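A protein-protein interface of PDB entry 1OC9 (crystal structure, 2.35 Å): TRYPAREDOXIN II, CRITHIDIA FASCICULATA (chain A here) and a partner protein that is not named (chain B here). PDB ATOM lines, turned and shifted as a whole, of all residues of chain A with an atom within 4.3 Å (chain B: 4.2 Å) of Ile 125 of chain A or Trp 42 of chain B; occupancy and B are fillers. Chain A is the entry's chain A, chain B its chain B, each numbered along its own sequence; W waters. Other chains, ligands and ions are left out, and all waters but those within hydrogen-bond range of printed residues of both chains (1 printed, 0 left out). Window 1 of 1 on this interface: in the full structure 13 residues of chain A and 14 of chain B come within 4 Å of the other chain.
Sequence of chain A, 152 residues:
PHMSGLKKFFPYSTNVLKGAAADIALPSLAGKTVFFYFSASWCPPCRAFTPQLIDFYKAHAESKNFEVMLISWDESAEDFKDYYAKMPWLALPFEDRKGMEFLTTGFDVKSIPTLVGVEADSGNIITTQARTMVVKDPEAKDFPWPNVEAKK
The side-chain sulfur (SG) of Cys 43 of chain B sits at hydrogen-bond distance from the backbone carbonyl oxygen (O) of Ile 112 of chain B, at 3.7 Å.
The backbone NH of Thr 128 of chain A lies within hydrogen-bond range of the side-chain carboxylate of Glu 149 of chain A (2.6 Å).
O of Ser 41 of chain B sits at hydrogen-bond distance from NH1 of Arg 47 of chain B, at 2.8 Å.
OE1 of Glu 149 of chain A sits at hydrogen-bond distance from OG1 of Thr 127 of chain A, at 3.0 Å.
The indole nitrogen of Trp 42 of chain B lies within hydrogen-bond range of the backbone carbonyl oxygen of Trp 73 of chain B (3.0 Å).
The backbone carbonyl oxygen of Gly 117 of chain A is in hydrogen-bond range of the backbone NH of Ile 126 of chain A, at 2.8 Å.
Water W1 lies within hydrogen-bond range of O of Asp 74 of chain B (2.8 Å) and O of Glu 149 of chain A (3.0 Å).
O of Gly 106 of chain A touches O of Trp 42 of chain B, 3.99 Å away.
CG of Pro 44 of chain B touches O of Gly 106 of chain A (3.5 Å).
O of Trp 42 of chain B touches CD1 of Phe 107 of chain A (3.6 Å).
Phe 107 of chain A touches Pro 44 of chain B.
Gly 123 of chain A touches Pro 45 of chain B.
CG2 of Ile 125 of chain A touches CZ3 of Trp 42 of chain B (3.4 Å).
SG of Cys 43 of chain B touches CG1 of Ile 125 of chain A, at 3.5 Å.
Ser 111 of chain B touches Ile 125 of chain A.
O of Ile 126 of chain A touches CZ3 of Trp 73 of chain B (3.6 Å).
O of Trp 73 of chain B touches CB of Glu 149 of chain A, 3.9 Å away.
Of the 11 printed residues of chain B, 8 touch a printed residue of chain A.
Hydrophobic or aromatic side chains of chain B that line the printed part of chain A: Trp 42, Pro 44, Pro 45, Trp 73 and Ile 112.
Of the 12 printed residues of chain A, 8 touch a printed residue of chain B.
Hydrophobic or aromatic side chains of chain A that line the printed part of chain B: Phe 107 and Ile 125.
Among the printed residues, no Asp or Glu carboxylate lies within 4 Å of a Lys or Arg side-chain nitrogen of the other chain.
Ile 125 of chain A touches six residues of chain B.
Of the printed residues of chain A, Trp 42 of chain B touches Gly 106 (3.99 Å), Phe 107 (3.6 Å), Ile 125 (3.4 Å), Thr 128 (3.6 Å) and Glu 149 (3.4 Å).
Of the printed residues of chain A, Cys 43 of chain B touches Ile 125 (3.5 Å).
Of the printed residues of chain A, Trp 73 of chain B touches Ile 126 and Glu 149.
Ser 41 of chain B touches none of the printed residues of chain A.
Thr 127 of chain A touches none of the printed residues of chain B.
The guanidinium group of Arg 47 of chain B lies within hydrogen-bond range of the backbone carbonyl oxygen of Gly 106 of chain A (2.8 Å).
ND2 of Asn 124 of chain A sits at hydrogen-bond distance from OG of Ser 111 of chain B (3.3 Å).
O of Ile 112 of chain B is in hydrogen-bond range of N of Ile 125 of chain A (2.9 Å).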
ATOM      1  N   PHE A   9       5.070   8.723  -9.351  1.00  0.00           N
ATOM      2  CA  PHE A   9       5.293  10.069  -9.871  1.00  0.00           C
ATOM      3  C   PHE A   9       6.781  10.469  -9.965  1.00  0.00           C
ATOM      4  O   PHE A   9       7.090  11.532 -10.465  1.00  0.00           O
ATOM      5  CB  PHE A   9       4.564  11.078  -9.015  1.00  0.00           C
ATOM      6  CG  PHE A   9       3.094  10.878  -8.986  1.00  0.00           C
ATOM      7  CD1 PHE A   9       2.331  11.045 -10.129  1.00  0.00           C
ATOM      8  CD2 PHE A   9       2.459  10.537  -7.811  1.00  0.00           C
ATOM      9  CE1 PHE A   9       0.918  10.826 -10.086  1.00  0.00           C
ATOM     10  CE2 PHE A   9       1.062  10.350  -7.766  1.00  0.00           C
ATOM     11  CZ  PHE A   9       0.317  10.480  -8.909  1.00  0.00           C
ATOM     12  N   GLY A 106       2.778  14.113 -17.979  1.00  0.00           N
ATOM     13  CA  GLY A 106       1.749  13.315 -17.383  1.00  0.00           C
ATOM     14  C   GLY A 106       0.441  13.991 -17.021  1.00  0.00           C
ATOM     15  O   GLY A 106      -0.621  13.434 -17.213  1.00  0.00           O
ATOM     16  N   PHE A 107       0.501  15.172 -16.444  1.00  0.00           N
ATOM     17  CA  PHE A 107      -0.707  15.840 -16.053  1.00  0.00           C
ATOM     18  C   PHE A 107      -1.133  16.873 -17.190  1.00  0.00           C
ATOM     19  O   PHE A 107      -2.112  17.587 -17.005  1.00  0.00           O
ATOM     20  CB  PHE A 107      -0.466  16.604 -14.765  1.00  0.00           C
ATOM     21  CG  PHE A 107      -0.338  15.753 -13.576  1.00  0.00           C
ATOM     22  CD1 PHE A 107      -1.399  15.038 -13.127  1.00  0.00           C
ATOM     23  CD2 PHE A 107       0.842  15.682 -12.894  1.00  0.00           C
ATOM     24  CE1 PHE A 107      -1.270  14.248 -12.042  1.00  0.00           C
ATOM     25  CE2 PHE A 107       0.971  14.865 -11.794  1.00  0.00           C
ATOM     26  CZ  PHE A 107      -0.073  14.189 -11.349  1.00  0.00           C
ATOM     27  N   GLY A 117      -3.459  18.170  -7.198  1.00  0.00           N
ATOM     28  CA  GLY A 117      -3.605  17.484  -5.929  1.00  0.00           C
ATOM     29  C   GLY A 117      -3.669  15.978  -6.119  1.00  0.00           C
ATOM     30  O   GLY A 117      -4.417  15.546  -7.000  1.00  0.00           O
ATOM     31  N   VAL A 118      -2.857  15.223  -5.357  1.00  0.00           N
ATOM     32  CA  VAL A 118      -2.854  13.779  -5.380  1.00  0.00           C
ATOM     33  C   VAL A 118      -2.898  13.194  -3.966  1.00  0.00           C
ATOM     34  O   VAL A 118      -2.571  13.839  -2.988  1.00  0.00           O
ATOM     35  CB  VAL A 118      -1.646  13.206  -6.119  1.00  0.00           C
ATOM     36  CG1 VAL A 118      -1.406  13.979  -7.422  1.00  0.00           C
ATOM     37  CG2 VAL A 118      -0.416  13.297  -5.292  1.00  0.00           C
ATOM     38  N   GLY A 123      -1.916   7.061  -4.539  1.00  0.00           N
ATOM     39  CA  GLY A 123      -1.285   7.598  -5.754  1.00  0.00           C
ATOM     40  C   GLY A 123      -2.320   8.101  -6.756  1.00  0.00           C
ATOM     41  O   GLY A 123      -1.989   8.453  -7.886  1.00  0.00           O
ATOM     42  N   ASN A 124      -3.562   8.220  -6.314  1.00  0.00           N
ATOM     43  CA  ASN A 124      -4.665   8.738  -7.144  1.00  0.00           C
ATOM     44  C   ASN A 124      -4.662  10.268  -7.324  1.00  0.00           C
ATOM     45  O   ASN A 124      -4.123  10.959  -6.497  1.00  0.00           O
ATOM     46  CB  ASN A 124      -5.993   8.346  -6.534  1.00  0.00           C
ATOM     47  CG  ASN A 124      -6.399   6.896  -6.861  1.00  0.00           C
ATOM     48  OD1 ASN A 124      -5.609   6.124  -7.404  1.00  0.00           O
ATOM     49  ND2 ASN A 124      -7.657   6.570  -6.607  1.00  0.00           N
ATOM     50  N   ILE A 125      -5.255  10.771  -8.410  1.00  0.00           N
ATOM     51  CA  ILE A 125      -5.342  12.165  -8.625  1.00  0.00           C
ATOM     52  C   ILE A 125      -6.704  12.727  -8.159  1.00  0.00           C
ATOM     53  O   ILE A 125      -7.752  12.157  -8.444  1.00  0.00           O
ATOM     54  CB  ILE A 125      -5.152  12.461 -10.132  1.00  0.00           C
ATOM     55  CG1 ILE A 125      -3.960  11.701 -10.753  1.00  0.00           C
ATOM     56  CG2 ILE A 125      -4.953  13.876 -10.296  1.00  0.00           C
ATOM     57  CD1 ILE A 125      -2.674  11.715  -9.930  1.00  0.00           C
ATOM     58  N   ILE A 126      -6.657  13.891  -7.507  1.00  0.00           N
ATOM     59  CA  ILE A 126      -7.804  14.559  -6.987  1.00  0.00           C
ATOM     60  C   ILE A 126      -8.233  15.640  -7.952  1.00  0.00           C
ATOM     61  O   ILE A 126      -9.422  15.691  -8.307  1.00  0.00           O
ATOM     62  CB  ILE A 126      -7.524  15.163  -5.616  1.00  0.00           C
ATOM     63  CG1 ILE A 126      -7.167  14.108  -4.587  1.00  0.00           C
ATOM     64  CG2 ILE A 126      -8.723  15.963  -5.126  1.00  0.00           C
ATOM     65  CD1 ILE A 126      -6.396  14.621  -3.369  1.00  0.00           C
ATOM     66  N   THR A 127      -7.307  16.519  -8.376  1.00  0.00           N
ATOM     67  CA  THR A 127      -7.641  17.611  -9.364  1.00  0.00           C
ATOM     68  C   THR A 127      -6.380  18.260  -9.935  1.00  0.00           C
ATOM     69  O   THR A 127      -5.334  18.268  -9.246  1.00  0.00           O
ATOM     70  CB  THR A 127      -8.551  18.660  -8.666  1.00  0.00           C
ATOM     71  OG1 THR A 127      -8.878  19.739  -9.527  1.00  0.00           O
ATOM     72  CG2 THR A 127      -7.816  19.330  -7.635  1.00  0.00           C
ATOM     73  N   THR A 128      -6.465  18.767 -11.169  1.00  0.00           N
ATOM     74  CA  THR A 128      -5.374  19.542 -11.737  1.00  0.00           C
ATOM     75  C   THR A 128      -5.681  21.041 -11.613  1.00  0.00           C
ATOM     76  O   THR A 128      -4.923  21.891 -12.070  1.00  0.00           O
ATOM     77  CB  THR A 128      -5.046  19.234 -13.191  1.00  0.00           C
ATOM     78  OG1 THR A 128      -6.169  19.526 -14.010  1.00  0.00           O
ATOM     79  CG2 THR A 128      -4.784  17.757 -13.402  1.00  0.00           C
ATOM     80  N   GLU A 149     -12.578  20.178 -12.270  1.00  0.00           N
ATOM     81  CA  GLU A 149     -12.716  20.133 -13.701  1.00  0.00           C
ATOM     82  C   GLU A 149     -14.191  20.045 -14.122  1.00  0.00           C
ATOM     83  O   GLU A 149     -14.531  20.346 -15.261  1.00  0.00           O
ATOM     84  CB  GLU A 149     -11.952  18.894 -14.237  1.00  0.00           C
ATOM     85  CG  GLU A 149     -10.401  19.003 -14.210  1.00  0.00           C
ATOM     86  CD  GLU A 149      -9.710  18.727 -12.855  1.00  0.00           C
ATOM     87  OE1 GLU A 149     -10.390  18.477 -11.790  1.00  0.00           O
ATOM     88  OE2 GLU A 149      -8.467  18.786 -12.826  1.00  0.00           O
ATOM     89  N   ALA B  40     -10.156  10.050 -16.463  1.00  0.00           N
ATOM     90  CA  ALA B  40      -9.987  11.268 -17.271  1.00  0.00           C
ATOM     91  C   ALA B  40      -8.621  11.238 -17.934  1.00  0.00           C
ATOM     92  O   ALA B  40      -7.660  10.597 -17.448  1.00  0.00           O
ATOM     93  CB  ALA B  40     -10.087  12.536 -16.387  1.00  0.00           C
ATOM     94  N   SER B  41      -8.499  11.987 -18.999  1.00  0.00           N
ATOM     95  CA  SER B  41      -7.272  12.001 -19.737  1.00  0.00           C
ATOM     96  C   SER B  41      -6.185  12.651 -18.985  1.00  0.00           C
ATOM     97  O   SER B  41      -5.046  12.417 -19.289  1.00  0.00           O
ATOM     98  CB  SER B  41      -7.425  12.732 -21.059  1.00  0.00           C
ATOM     99  OG  SER B  41      -7.629  14.092 -20.758  1.00  0.00           O
ATOM    100  N   TRP B  42      -6.524  13.484 -18.019  1.00  0.00           N
ATOM    101  CA  TRP B  42      -5.479  14.145 -17.286  1.00  0.00           C
ATOM    102  C   TRP B  42      -4.848  13.352 -16.118  1.00  0.00           C
ATOM    103  O   TRP B  42      -4.093  13.933 -15.307  1.00  0.00           O
ATOM    104  CB  TRP B  42      -5.990  15.486 -16.768  1.00  0.00           C
ATOM    105  CG  TRP B  42      -7.337  15.531 -16.107  1.00  0.00           C
ATOM    106  CD1 TRP B  42      -8.517  15.871 -16.701  1.00  0.00           C
ATOM    107  CD2 TRP B  42      -7.645  15.274 -14.735  1.00  0.00           C
ATOM    108  NE1 TRP B  42      -9.535  15.848 -15.789  1.00  0.00           N
ATOM    109  CE2 TRP B  42      -9.037  15.464 -14.575  1.00  0.00           C
ATOM    110  CE3 TRP B  42      -6.894  14.886 -13.633  1.00  0.00           C
ATOM    111  CZ2 TRP B  42      -9.678  15.314 -13.354  1.00  0.00           C
ATOM    112  CZ3 TRP B  42      -7.516  14.714 -12.439  1.00  0.00           C
ATOM    113  CH2 TRP B  42      -8.895  14.917 -12.295  1.00  0.00           C
ATOM    114  N   CYS B  43      -5.134  12.064 -16.042  1.00  0.00           N
ATOM    115  CA  CYS B  43      -4.746  11.265 -14.901  1.00  0.00           C
ATOM    116  C   CYS B  43      -3.736  10.177 -15.214  1.00  0.00           C
ATOM    117  O   CYS B  43      -4.053   9.201 -15.823  1.00  0.00           O
ATOM    118  CB  CYS B  43      -6.034  10.651 -14.298  1.00  0.00           C
ATOM    119  SG  CYS B  43      -5.751   9.578 -12.918  1.00  0.00           S
ATOM    120  N   PRO B  44      -2.503  10.349 -14.775  1.00  0.00           N
ATOM    121  CA  PRO B  44      -1.448   9.361 -15.019  1.00  0.00           C
ATOM    122  C   PRO B  44      -1.770   7.932 -14.542  1.00  0.00           C
ATOM    123  O   PRO B  44      -1.633   6.999 -15.290  1.00  0.00           O
ATOM    124  CB  PRO B  44      -0.237   9.967 -14.294  1.00  0.00           C
ATOM    125  CG  PRO B  44      -0.508  11.450 -14.340  1.00  0.00           C
ATOM    126  CD  PRO B  44      -1.982  11.536 -14.068  1.00  0.00           C
ATOM    127  N   PRO B  45      -2.187   7.744 -13.320  1.00  0.00           N
ATOM    128  CA  PRO B  45      -2.506   6.381 -12.860  1.00  0.00           C
ATOM    129  C   PRO B  45      -3.630   5.787 -13.715  1.00  0.00           C
ATOM    130  O   PRO B  45      -3.572   4.603 -14.052  1.00  0.00           O
ATOM    131  CB  PRO B  45      -2.846   6.563 -11.357  1.00  0.00           C
ATOM    132  CG  PRO B  45      -3.170   8.047 -11.233  1.00  0.00           C
ATOM    133  CD  PRO B  45      -2.261   8.756 -12.242  1.00  0.00           C
ATOM    134  N   ARG B  47      -4.102   6.506 -16.887  1.00  0.00           N
ATOM    135  CA  ARG B  47      -3.448   6.158 -18.144  1.00  0.00           C
ATOM    136  C   ARG B  47      -2.656   4.830 -18.015  1.00  0.00           C
ATOM    137  O   ARG B  47      -2.547   4.075 -18.969  1.00  0.00           O
ATOM    138  CB  ARG B  47      -2.602   7.341 -18.599  1.00  0.00           C
ATOM    139  CG  ARG B  47      -2.316   7.444 -20.089  1.00  0.00           C
ATOM    140  CD  ARG B  47      -1.627   8.792 -20.465  1.00  0.00           C
ATOM    141  NE  ARG B  47      -2.329   9.931 -19.864  1.00  0.00           N
ATOM    142  CZ  ARG B  47      -1.819  10.707 -18.908  1.00  0.00           C
ATOM    143  NH1 ARG B  47      -2.514  11.686 -18.367  1.00  0.00           N
ATOM    144  NH2 ARG B  47      -0.584  10.477 -18.487  1.00  0.00           N
ATOM    145  N   TRP B  73     -14.329  12.373 -15.882  1.00  0.00           N
ATOM    146  CA  TRP B  73     -13.957  13.577 -15.155  1.00  0.00           C
ATOM    147  C   TRP B  73     -13.163  14.482 -16.133  1.00  0.00           C
ATOM    148  O   TRP B  73     -12.442  15.318 -15.703  1.00  0.00           O
ATOM    149  CB  TRP B  73     -13.073  13.275 -13.932  1.00  0.00           C
ATOM    150  CG  TRP B  73     -13.779  12.913 -12.723  1.00  0.00           C
ATOM    151  CD1 TRP B  73     -15.063  12.412 -12.617  1.00  0.00           C
ATOM    152  CD2 TRP B  73     -13.263  12.955 -11.397  1.00  0.00           C
ATOM    153  NE1 TRP B  73     -15.385  12.240 -11.300  1.00  0.00           N
ATOM    154  CE2 TRP B  73     -14.293  12.525 -10.533  1.00  0.00           C
ATOM    155  CE3 TRP B  73     -12.033  13.333 -10.847  1.00  0.00           C
ATOM    156  CZ2 TRP B  73     -14.118  12.413  -9.188  1.00  0.00           C
ATOM    157  CZ3 TRP B  73     -11.881  13.299  -9.552  1.00  0.00           C
ATOM    158  CH2 TRP B  73     -12.911  12.817  -8.695  1.00  0.00           C
ATOM    159  N   ASP B  74     -13.265  14.278 -17.432  1.00  0.00           N
ATOM    160  CA  ASP B  74     -12.616  15.188 -18.387  1.00  0.00           C
ATOM    161  C   ASP B  74     -13.108  16.639 -18.277  1.00  0.00           C
ATOM    162  O   ASP B  74     -14.188  16.900 -17.799  1.00  0.00           O
ATOM    163  CB  ASP B  74     -12.731  14.673 -19.810  1.00  0.00           C
ATOM    164  CG  ASP B  74     -11.954  13.417 -19.995  1.00  0.00           C
ATOM    165  OD1 ASP B  74     -10.717  13.482 -19.860  1.00  0.00           O
ATOM    166  OD2 ASP B  74     -12.495  12.312 -20.182  1.00  0.00           O
ATOM    167  N   SER B 111     -11.360  10.681  -5.839  1.00  0.00           N
ATOM    168  CA  SER B 111     -10.162  10.749  -6.663  1.00  0.00           C
ATOM    169  C   SER B 111     -10.215   9.638  -7.698  1.00  0.00           C
ATOM    170  O   SER B 111     -11.055   8.731  -7.599  1.00  0.00           O
ATOM    171  CB  SER B 111      -8.918  10.563  -5.792  1.00  0.00           C
ATOM    172  OG  SER B 111      -8.899   9.282  -5.155  1.00  0.00           O
ATOM    173  N   ILE B 112      -9.370   9.706  -8.723  1.00  0.00           N
ATOM    174  CA  ILE B 112      -9.368   8.715  -9.769  1.00  0.00           C
ATOM    175  C   ILE B 112      -7.996   8.119 -10.004  1.00  0.00           C
ATOM    176  O   ILE B 112      -7.014   8.718  -9.580  1.00  0.00           O
ATOM    177  CB  ILE B 112      -9.893   9.349 -11.060  1.00  0.00           C
ATOM    178  CG1 ILE B 112      -9.115  10.603 -11.411  1.00  0.00           C
ATOM    179  CG2 ILE B 112     -11.400   9.739 -10.933  1.00  0.00           C
ATOM    180  CD1 ILE B 112      -9.548  11.123 -12.776  1.00  0.00           C
HETATM  181  O   HOH W   1     -16.257  18.714 -17.086  1.00  0.00           O
